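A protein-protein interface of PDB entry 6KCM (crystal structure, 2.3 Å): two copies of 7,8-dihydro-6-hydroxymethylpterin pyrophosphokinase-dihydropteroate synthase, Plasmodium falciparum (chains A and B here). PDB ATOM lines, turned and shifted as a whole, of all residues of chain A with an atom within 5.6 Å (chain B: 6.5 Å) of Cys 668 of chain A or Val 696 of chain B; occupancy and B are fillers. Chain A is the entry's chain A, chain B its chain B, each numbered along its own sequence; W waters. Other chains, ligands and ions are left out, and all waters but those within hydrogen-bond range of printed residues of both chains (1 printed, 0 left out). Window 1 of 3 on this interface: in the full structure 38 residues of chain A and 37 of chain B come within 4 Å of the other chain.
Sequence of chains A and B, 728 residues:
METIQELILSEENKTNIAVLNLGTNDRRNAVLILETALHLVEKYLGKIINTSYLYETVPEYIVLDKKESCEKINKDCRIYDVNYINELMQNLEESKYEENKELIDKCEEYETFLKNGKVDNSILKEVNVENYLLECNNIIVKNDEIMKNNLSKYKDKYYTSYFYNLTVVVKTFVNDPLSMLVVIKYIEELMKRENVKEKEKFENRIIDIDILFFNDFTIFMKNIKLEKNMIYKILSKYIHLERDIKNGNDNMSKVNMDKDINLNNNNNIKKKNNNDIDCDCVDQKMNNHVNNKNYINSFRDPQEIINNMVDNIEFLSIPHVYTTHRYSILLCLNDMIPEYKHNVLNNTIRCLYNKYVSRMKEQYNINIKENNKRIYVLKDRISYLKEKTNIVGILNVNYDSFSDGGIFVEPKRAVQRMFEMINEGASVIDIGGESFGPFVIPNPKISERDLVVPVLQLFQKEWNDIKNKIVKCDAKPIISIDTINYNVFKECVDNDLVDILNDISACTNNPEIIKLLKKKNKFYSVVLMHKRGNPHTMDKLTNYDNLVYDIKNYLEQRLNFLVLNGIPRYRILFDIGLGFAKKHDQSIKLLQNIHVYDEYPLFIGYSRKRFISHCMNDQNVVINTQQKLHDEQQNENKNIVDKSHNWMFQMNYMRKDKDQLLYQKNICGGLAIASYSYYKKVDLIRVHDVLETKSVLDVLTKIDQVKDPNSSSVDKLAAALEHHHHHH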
ATOM      1  N   MET A 616      17.600 -18.318  24.040  1.00  0.00           N
ATOM      2  CA  MET A 616      18.539 -17.274  24.464  1.00  0.00           C
ATOM      3  C   MET A 616      17.925 -16.470  25.607  1.00  0.00           C
ATOM      4  O   MET A 616      16.830 -15.920  25.467  1.00  0.00           O
ATOM      5  CB  MET A 616      18.903 -16.322  23.307  1.00  0.00           C
ATOM      6  CG  MET A 616      19.588 -16.934  22.076  1.00  0.00           C
ATOM      7  SD  MET A 616      20.862 -18.141  22.485  1.00  0.00           S
ATOM      8  CE  MET A 616      21.298 -18.868  20.937  1.00  0.00           C
ATOM      9  N   TYR A 663      21.389 -12.939  14.971  1.00  0.00           N
ATOM     10  CA  TYR A 663      21.848 -13.840  13.945  1.00  0.00           C
ATOM     11  C   TYR A 663      23.070 -14.672  14.414  1.00  0.00           C
ATOM     12  O   TYR A 663      23.152 -15.901  14.160  1.00  0.00           O
ATOM     13  CB  TYR A 663      22.109 -12.968  12.708  1.00  0.00           C
ATOM     14  CG  TYR A 663      22.792 -13.567  11.512  1.00  0.00           C
ATOM     15  CD1 TYR A 663      22.191 -14.572  10.745  1.00  0.00           C
ATOM     16  CD2 TYR A 663      24.018 -13.060  11.087  1.00  0.00           C
ATOM     17  CE1 TYR A 663      22.833 -15.089   9.618  1.00  0.00           C
ATOM     18  CE2 TYR A 663      24.664 -13.566   9.969  1.00  0.00           C
ATOM     19  CZ  TYR A 663      24.077 -14.577   9.240  1.00  0.00           C
ATOM     20  OH  TYR A 663      24.750 -15.054   8.142  1.00  0.00           O
ATOM     21  N   GLN A 664      24.002 -14.028  15.123  1.00  0.00           N
ATOM     22  CA  GLN A 664      25.174 -14.740  15.583  1.00  0.00           C
ATOM     23  C   GLN A 664      24.859 -15.649  16.775  1.00  0.00           C
ATOM     24  O   GLN A 664      25.360 -16.765  16.833  1.00  0.00           O
ATOM     25  CB  GLN A 664      26.383 -13.829  15.865  1.00  0.00           C
ATOM     26  CG  GLN A 664      27.692 -14.653  15.799  1.00  0.00           C
ATOM     27  CD  GLN A 664      28.970 -13.895  16.144  1.00  0.00           C
ATOM     28  OE1 GLN A 664      29.018 -13.128  17.103  1.00  0.00           O
ATOM     29  NE2 GLN A 664      30.024 -14.132  15.360  1.00  0.00           N
ATOM     30  N   LYS A 665      24.015 -15.179  17.692  1.00  0.00           N
ATOM     31  CA  LYS A 665      23.551 -16.010  18.786  1.00  0.00           C
ATOM     32  C   LYS A 665      22.884 -17.277  18.234  1.00  0.00           C
ATOM     33  O   LYS A 665      23.164 -18.379  18.706  1.00  0.00           O
ATOM     34  CB  LYS A 665      22.609 -15.226  19.712  1.00  0.00           C
ATOM     35  CG  LYS A 665      23.321 -14.116  20.490  1.00  0.00           C
ATOM     36  CD  LYS A 665      22.513 -13.562  21.663  1.00  0.00           C
ATOM     37  CE  LYS A 665      22.354 -14.570  22.814  1.00  0.00           C
ATOM     38  NZ  LYS A 665      23.558 -15.020  23.601  1.00  0.00           N
ATOM     39  N   ASN A 666      22.087 -17.118  17.171  1.00  0.00           N
ATOM     40  CA  ASN A 666      21.352 -18.228  16.581  1.00  0.00           C
ATOM     41  C   ASN A 666      22.321 -19.210  15.934  1.00  0.00           C
ATOM     42  O   ASN A 666      22.210 -20.416  16.114  1.00  0.00           O
ATOM     43  CB  ASN A 666      20.226 -17.744  15.628  1.00  0.00           C
ATOM     44  CG  ASN A 666      19.400 -18.890  15.054  1.00  0.00           C
ATOM     45  OD1 ASN A 666      19.908 -19.736  14.304  1.00  0.00           O
ATOM     46  ND2 ASN A 666      18.122 -18.932  15.397  1.00  0.00           N
ATOM     47  N   ILE A 667      23.286 -18.705  15.198  1.00  0.00           N
ATOM     48  CA  ILE A 667      24.241 -19.617  14.608  1.00  0.00           C
ATOM     49  C   ILE A 667      24.993 -20.378  15.709  1.00  0.00           C
ATOM     50  O   ILE A 667      25.208 -21.591  15.575  1.00  0.00           O
ATOM     51  CB  ILE A 667      25.229 -18.887  13.700  1.00  0.00           C
ATOM     52  CG1 ILE A 667      24.477 -18.325  12.493  1.00  0.00           C
ATOM     53  CG2 ILE A 667      26.387 -19.823  13.311  1.00  0.00           C
ATOM     54  CD1 ILE A 667      25.208 -17.195  11.769  1.00  0.00           C
ATOM     55  N   CYS A 668      25.364 -19.688  16.799  1.00  0.00           N
ATOM     56  CA  CYS A 668      26.084 -20.348  17.877  1.00  0.00           C
ATOM     57  C   CYS A 668      25.184 -21.333  18.656  1.00  0.00           C
ATOM     58  O   CYS A 668      25.642 -22.428  19.060  1.00  0.00           O
ATOM     59  CB  CYS A 668      26.781 -19.332  18.789  1.00  0.00           C
ATOM     60  SG  CYS A 668      28.058 -18.386  17.906  1.00  0.00           S
ATOM     61  N   GLY A 669      23.912 -20.951  18.832  1.00  0.00           N
ATOM     62  CA  GLY A 669      22.923 -21.819  19.460  1.00  0.00           C
ATOM     63  C   GLY A 669      22.817 -23.111  18.671  1.00  0.00           C
ATOM     64  O   GLY A 669      22.686 -24.171  19.235  1.00  0.00           O
ATOM     65  N   GLY A 670      22.941 -23.037  17.353  1.00  0.00           N
ATOM     66  CA  GLY A 670      22.923 -24.235  16.546  1.00  0.00           C
ATOM     67  C   GLY A 670      24.135 -25.135  16.733  1.00  0.00           C
ATOM     68  O   GLY A 670      24.036 -26.358  16.562  1.00  0.00           O
ATOM     69  N   LEU A 671      25.285 -24.545  17.075  1.00  0.00           N
ATOM     70  CA  LEU A 671      26.517 -25.325  17.307  1.00  0.00           C
ATOM     71  C   LEU A 671      26.393 -26.153  18.564  1.00  0.00           C
ATOM     72  O   LEU A 671      26.928 -27.241  18.614  1.00  0.00           O
ATOM     73  CB  LEU A 671      27.767 -24.429  17.340  1.00  0.00           C
ATOM     74  CG  LEU A 671      28.060 -23.816  15.944  1.00  0.00           C
ATOM     75  CD1 LEU A 671      29.183 -22.788  16.094  1.00  0.00           C
ATOM     76  CD2 LEU A 671      28.357 -24.840  14.834  1.00  0.00           C
ATOM     77  N   ALA A 672      25.663 -25.633  19.552  1.00  0.00           N
ATOM     78  CA  ALA A 672      25.220 -26.379  20.726  1.00  0.00           C
ATOM     79  C   ALA A 672      24.417 -27.620  20.331  1.00  0.00           C
ATOM     80  O   ALA A 672      24.662 -28.718  20.868  1.00  0.00           O
ATOM     81  CB  ALA A 672      24.375 -25.494  21.645  1.00  0.00           C
ATOM     82  N   ILE A 673      23.476 -27.464  19.387  1.00  0.00           N
ATOM     83  CA  ILE A 673      22.655 -28.597  18.919  1.00  0.00           C
ATOM     84  C   ILE A 673      23.506 -29.533  18.058  1.00  0.00           C
ATOM     85  O   ILE A 673      23.309 -30.738  18.079  1.00  0.00           O
ATOM     86  CB  ILE A 673      21.372 -28.143  18.164  1.00  0.00           C
ATOM     87  CG1 ILE A 673      20.611 -27.113  19.017  1.00  0.00           C
ATOM     88  CG2 ILE A 673      20.489 -29.340  17.791  1.00  0.00           C
ATOM     89  CD1 ILE A 673      19.269 -26.669  18.457  1.00  0.00           C
ATOM     90  N   MET B 648      33.525 -14.704  13.926  1.00  0.00           N
ATOM     91  CA  MET B 648      33.553 -14.717  15.391  1.00  0.00           C
ATOM     92  C   MET B 648      34.801 -14.050  15.997  1.00  0.00           C
ATOM     93  O   MET B 648      34.854 -13.763  17.208  1.00  0.00           O
ATOM     94  CB  MET B 648      33.380 -16.143  15.891  1.00  0.00           C
ATOM     95  CG  MET B 648      32.027 -16.732  15.538  1.00  0.00           C
ATOM     96  SD  MET B 648      31.911 -18.491  15.913  1.00  0.00           S
ATOM     97  CE  MET B 648      33.077 -19.174  14.762  1.00  0.00           C
ATOM     98  N   LEU B 671      33.896 -23.705  21.140  1.00  0.00           N
ATOM     99  CA  LEU B 671      32.459 -23.852  21.456  1.00  0.00           C
ATOM    100  C   LEU B 671      32.102 -25.324  21.628  1.00  0.00           C
ATOM    101  O   LEU B 671      31.263 -25.673  22.459  1.00  0.00           O
ATOM    102  CB  LEU B 671      31.556 -23.186  20.395  1.00  0.00           C
ATOM    103  CG  LEU B 671      31.641 -21.664  20.289  1.00  0.00           C
ATOM    104  CD1 LEU B 671      30.769 -21.199  19.107  1.00  0.00           C
ATOM    105  CD2 LEU B 671      31.245 -21.006  21.623  1.00  0.00           C
ATOM    106  N   ALA B 672      32.774 -26.193  20.877  1.00  0.00           N
ATOM    107  CA  ALA B 672      32.700 -27.629  21.155  1.00  0.00           C
ATOM    108  C   ALA B 672      33.213 -27.969  22.585  1.00  0.00           C
ATOM    109  O   ALA B 672      32.589 -28.778  23.310  1.00  0.00           O
ATOM    110  CB  ALA B 672      33.469 -28.406  20.097  1.00  0.00           C
ATOM    111  N   ALA B 674      33.297 -25.881  25.096  1.00  0.00           N
ATOM    112  CA  ALA B 674      32.230 -25.350  25.982  1.00  0.00           C
ATOM    113  C   ALA B 674      31.107 -26.379  26.227  1.00  0.00           C
ATOM    114  O   ALA B 674      30.592 -26.493  27.351  1.00  0.00           O
ATOM    115  CB  ALA B 674      31.631 -24.064  25.414  1.00  0.00           C
ATOM    116  N   SER B 675      30.725 -27.104  25.172  1.00  0.00           N
ATOM    117  CA  SER B 675      29.628 -28.114  25.238  1.00  0.00           C
ATOM    118  C   SER B 675      30.065 -29.306  26.094  1.00  0.00           C
ATOM    119  O   SER B 675      29.337 -29.758  26.980  1.00  0.00           O
ATOM    120  CB  SER B 675      29.283 -28.670  23.841  1.00  0.00           C
ATOM    121  OG  SER B 675      28.834 -27.656  22.948  1.00  0.00           O
ATOM    122  N   TYR B 678      30.193 -28.182  29.588  1.00  0.00           N
ATOM    123  CA  TYR B 678      28.826 -28.198  30.093  1.00  0.00           C
ATOM    124  C   TYR B 678      28.442 -29.607  30.548  1.00  0.00           C
ATOM    125  O   TYR B 678      27.970 -29.801  31.674  1.00  0.00           O
ATOM    126  CB  TYR B 678      27.810 -27.697  29.043  1.00  0.00           C
ATOM    127  CG  TYR B 678      26.396 -27.814  29.560  1.00  0.00           C
ATOM    128  CD1 TYR B 678      25.826 -26.791  30.325  1.00  0.00           C
ATOM    129  CD2 TYR B 678      25.662 -28.963  29.347  1.00  0.00           C
ATOM    130  CE1 TYR B 678      24.533 -26.905  30.838  1.00  0.00           C
ATOM    131  CE2 TYR B 678      24.375 -29.090  29.830  1.00  0.00           C
ATOM    132  CZ  TYR B 678      23.820 -28.066  30.568  1.00  0.00           C
ATOM    133  OH  TYR B 678      22.563 -28.221  31.067  1.00  0.00           O
ATOM    134  N   LEU B 691      29.628 -13.914  24.008  1.00  0.00           N
ATOM    135  CA  LEU B 691      28.308 -14.050  23.360  1.00  0.00           C
ATOM    136  C   LEU B 691      28.109 -15.450  22.784  1.00  0.00           C
ATOM    137  O   LEU B 691      27.101 -16.089  23.014  1.00  0.00           O
ATOM    138  CB  LEU B 691      28.161 -12.994  22.237  1.00  0.00           C
ATOM    139  CG  LEU B 691      26.936 -13.096  21.317  1.00  0.00           C
ATOM    140  CD1 LEU B 691      26.408 -11.702  20.943  1.00  0.00           C
ATOM    141  CD2 LEU B 691      27.214 -13.960  20.057  1.00  0.00           C
ATOM    142  N   GLU B 692      29.084 -15.900  22.021  1.00  0.00           N
ATOM    143  CA  GLU B 692      29.048 -17.204  21.383  1.00  0.00           C
ATOM    144  C   GLU B 692      28.895 -18.306  22.410  1.00  0.00           C
ATOM    145  O   GLU B 692      28.102 -19.214  22.236  1.00  0.00           O
ATOM    146  CB  GLU B 692      30.354 -17.411  20.644  1.00  0.00           C
ATOM    147  CG  GLU B 692      30.552 -16.431  19.506  1.00  0.00           C
ATOM    148  CD  GLU B 692      31.392 -15.229  19.897  1.00  0.00           C
ATOM    149  OE1 GLU B 692      31.150 -14.572  20.936  1.00  0.00           O
ATOM    150  OE2 GLU B 692      32.326 -14.946  19.150  1.00  0.00           O
ATOM    151  N   THR B 693      29.654 -18.196  23.500  1.00  0.00           N
ATOM    152  CA  THR B 693      29.737 -19.240  24.496  1.00  0.00           C
ATOM    153  C   THR B 693      28.452 -19.268  25.270  1.00  0.00           C
ATOM    154  O   THR B 693      27.926 -20.347  25.549  1.00  0.00           O
ATOM    155  CB  THR B 693      30.959 -19.029  25.428  1.00  0.00           C
ATOM    156  OG1 THR B 693      32.138 -19.041  24.630  1.00  0.00           O
ATOM    157  CG2 THR B 693      31.069 -20.145  26.496  1.00  0.00           C
ATOM    158  N   LYS B 694      27.940 -18.086  25.624  1.00  0.00           N
ATOM    159  CA  LYS B 694      26.641 -17.997  26.311  1.00  0.00           C
ATOM    160  C   LYS B 694      25.464 -18.560  25.456  1.00  0.00           C
ATOM    161  O   LYS B 694      24.527 -19.160  25.988  1.00  0.00           O
ATOM    162  CB  LYS B 694      26.369 -16.546  26.699  1.00  0.00           C
ATOM    163  CG  LYS B 694      25.188 -16.341  27.636  1.00  0.00           C
ATOM    164  CD  LYS B 694      25.409 -16.998  28.997  1.00  0.00           C
ATOM    165  CE  LYS B 694      24.319 -16.642  30.006  1.00  0.00           C
ATOM    166  NZ  LYS B 694      22.965 -16.605  29.390  1.00  0.00           N
ATOM    167  N   SER B 695      25.522 -18.367  24.143  1.00  0.00           N
ATOM    168  CA  SER B 695      24.478 -18.902  23.243  1.00  0.00           C
ATOM    169  C   SER B 695      24.468 -20.443  23.285  1.00  0.00           C
ATOM    170  O   SER B 695      23.407 -21.077  23.396  1.00  0.00           O
ATOM    171  CB  SER B 695      24.712 -18.376  21.826  1.00  0.00           C
ATOM    172  OG  SER B 695      24.704 -16.948  21.818  1.00  0.00           O
ATOM    173  N   VAL B 696      25.666 -21.041  23.262  1.00  0.00           N
ATOM    174  CA  VAL B 696      25.826 -22.479  23.462  1.00  0.00           C
ATOM    175  C   VAL B 696      25.276 -22.931  24.806  1.00  0.00           C
ATOM    176  O   VAL B 696      24.476 -23.865  24.860  1.00  0.00           O
ATOM    177  CB  VAL B 696      27.298 -22.923  23.251  1.00  0.00           C
ATOM    178  CG1 VAL B 696      27.516 -24.374  23.674  1.00  0.00           C
ATOM    179  CG2 VAL B 696      27.682 -22.741  21.782  1.00  0.00           C
ATOM    180  N   LEU B 697      25.658 -22.262  25.892  1.00  0.00           N
ATOM    181  CA  LEU B 697      25.246 -22.746  27.207  1.00  0.00           C
ATOM    182  C   LEU B 697      23.735 -22.604  27.414  1.00  0.00           C
ATOM    183  O   LEU B 697      23.107 -23.433  28.095  1.00  0.00           O
ATOM    184  CB  LEU B 697      26.051 -22.087  28.346  1.00  0.00           C
ATOM    185  CG  LEU B 697      27.601 -22.238  28.402  1.00  0.00           C
ATOM    186  CD1 LEU B 697      28.170 -21.569  29.642  1.00  0.00           C
ATOM    187  CD2 LEU B 697      28.067 -23.682  28.405  1.00  0.00           C
ATOM    188  N   ASP B 698      23.146 -21.550  26.857  1.00  0.00           N
ATOM    189  CA  ASP B 698      21.702 -21.347  26.995  1.00  0.00           C
ATOM    190  C   ASP B 698      20.922 -22.455  26.284  1.00  0.00           C
ATOM    191  O   ASP B 698      19.986 -22.987  26.831  1.00  0.00           O
ATOM    192  CB  ASP B 698      21.281 -19.978  26.454  1.00  0.00           C
ATOM    193  CG  ASP B 698      21.627 -18.818  27.413  1.00  0.00           C
ATOM    194  OD1 ASP B 698      21.963 -19.038  28.616  1.00  0.00           O
ATOM    195  OD2 ASP B 698      21.562 -17.662  26.948  1.00  0.00           O
ATOM    196  N   VAL B 699      21.338 -22.822  25.075  1.00  0.00           N
ATOM    197  CA  VAL B 699      20.672 -23.889  24.360  1.00  0.00           C
ATOM    198  C   VAL B 699      20.842 -25.236  25.072  1.00  0.00           C
ATOM    199  O   VAL B 699      19.862 -25.970  25.252  1.00  0.00           O
ATOM    200  CB  VAL B 699      21.165 -23.971  22.900  1.00  0.00           C
ATOM    201  CG1 VAL B 699      20.610 -25.221  22.206  1.00  0.00           C
ATOM    202  CG2 VAL B 699      20.833 -22.684  22.125  1.00  0.00           C
ATOM    203  N   LEU B 700      22.060 -25.578  25.495  1.00  0.00           N
ATOM    204  CA  LEU B 700      22.257 -26.865  26.186  1.00  0.00           C
ATOM    205  C   LEU B 700      21.459 -26.940  27.481  1.00  0.00           C
ATOM    206  O   LEU B 700      20.880 -27.977  27.798  1.00  0.00           O
ATOM    207  CB  LEU B 700      23.731 -27.173  26.431  1.00  0.00           C
ATOM    208  CG  LEU B 700      24.629 -27.243  25.176  1.00  0.00           C
ATOM    209  CD1 LEU B 700      26.070 -27.401  25.596  1.00  0.00           C
ATOM    210  CD2 LEU B 700      24.268 -28.409  24.259  1.00  0.00           C
ATOM    211  N   THR B 701      21.409 -25.831  28.216  1.00  0.00           N
ATOM    212  CA  THR B 701      20.653 -25.749  29.462  1.00  0.00           C
ATOM    213  C   THR B 701      19.153 -25.954  29.186  1.00  0.00           C
ATOM    214  O   THR B 701      18.482 -26.697  29.897  1.00  0.00           O
ATOM    215  CB  THR B 701      20.916 -24.392  30.169  1.00  0.00           C
ATOM    216  OG1 THR B 701      22.318 -24.298  30.508  1.00  0.00           O
ATOM    217  CG2 THR B 701      20.084 -24.264  31.451  1.00  0.00           C
HETATM  218  O   HOH W   1      22.153 -15.805  25.455  1.00  0.00           O
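The side-chain amino group (NZ) of Lys 665 of chain A lies within hydrogen-bond range of the side-chain hydroxyl (OG) of Ser 695 of chain B (2.9 Å).
The side-chain sulfur (SG) of Cys 668 of chain A is in hydrogen-bond range of the backbone carbonyl oxygen (O) of Gln 664 of chain A. The backbone carbonyl oxygen of Leu 671 of chain B is in hydrogen-bond range of the side-chain hydroxyl of Ser 675 of chain B. The side-chain hydroxyl (OG) of Ser 695 of chain B lies within hydrogen-bond range of the backbone carbonyl oxygen (O) of Leu 691 of chain B (2.8 Å). NZ of Lys 694 of chain B is in salt-bridge range of OD1 of Asp 698 of chain B.
CB of Ser 695 of chain B touches CE of Met 616 of chain A, 3.6 Å away. OD2 of Asp 698 of chain B touches CA of Met 616 of chain A, at 3.9 Å. Met 648 of chain B touches Gln 664 of chain A (CG to NE2, 3.3 Å). Gln 664 of chain A touches Leu 691 of chain B (OE1 to CD2, 3.6 Å). Cys 668 of chain A touches Glu 692 of chain B. Val 696 of chain B touches Cys 668 of chain A. Leu 671 of chain B touches Leu 671 of chain A. Ala 672 of chain A touches Val 696 of chain B (CB to O, 3.6 Å). Val 699 of chain B touches Ala 672 of chain A (CB to CB, 3.8 Å). Val 699 of chain B touches Ile 673 of chain A.
Of chain B, only Glu 692 (3.5 Å), Ser 695 (3.8 Å) and Val 696 (3.4 Å) come within 4 Å of Cys 668 of chain A. Of chain A, only Cys 668 and Ala 672 come within 4 Å of Val 696 of chain B. Of the printed residues of chain B, Leu 671 of chain A touches Leu 671 (3.8 Å). Printed residues of chain A within 4 Å of Glu 692 of chain B: Cys 668 (3.5 Å). Printed residues of chain B within 4 Å of Lys 665 of chain A: Leu 691 and Ser 695. Thr 693 of chain B touches none of the printed residues of chain A. Asn 666 of chain A touches none of the printed residues of chain B. The nearest residue of chain B that does not touch Cys 668 of chain A is Leu 671 of chain B (4.1 Å). The nearest printed residue of chain A that does not touch Val 696 of chain B is Gly 669 of chain A (4.8 Å).
Hydrophobic or aromatic side chains of chain B within 4 Å of the printed part of chain A: Met 648, Leu 671, Leu 691, Val 696, Val 699 and Leu 700. Hydrophobic or aromatic side chains of chain A within 4 Å of the printed part of chain B: Met 616, Leu 671, Ala 672 and Ile 673.
Leu 671 of chain B touches its own counterpart, Leu 671 of chain A.
Water W1 lies within hydrogen-bond range of OD2 of Asp 698 of chain B (2.5 Å) and NZ of Lys 665 of chain A (2.5 Å).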
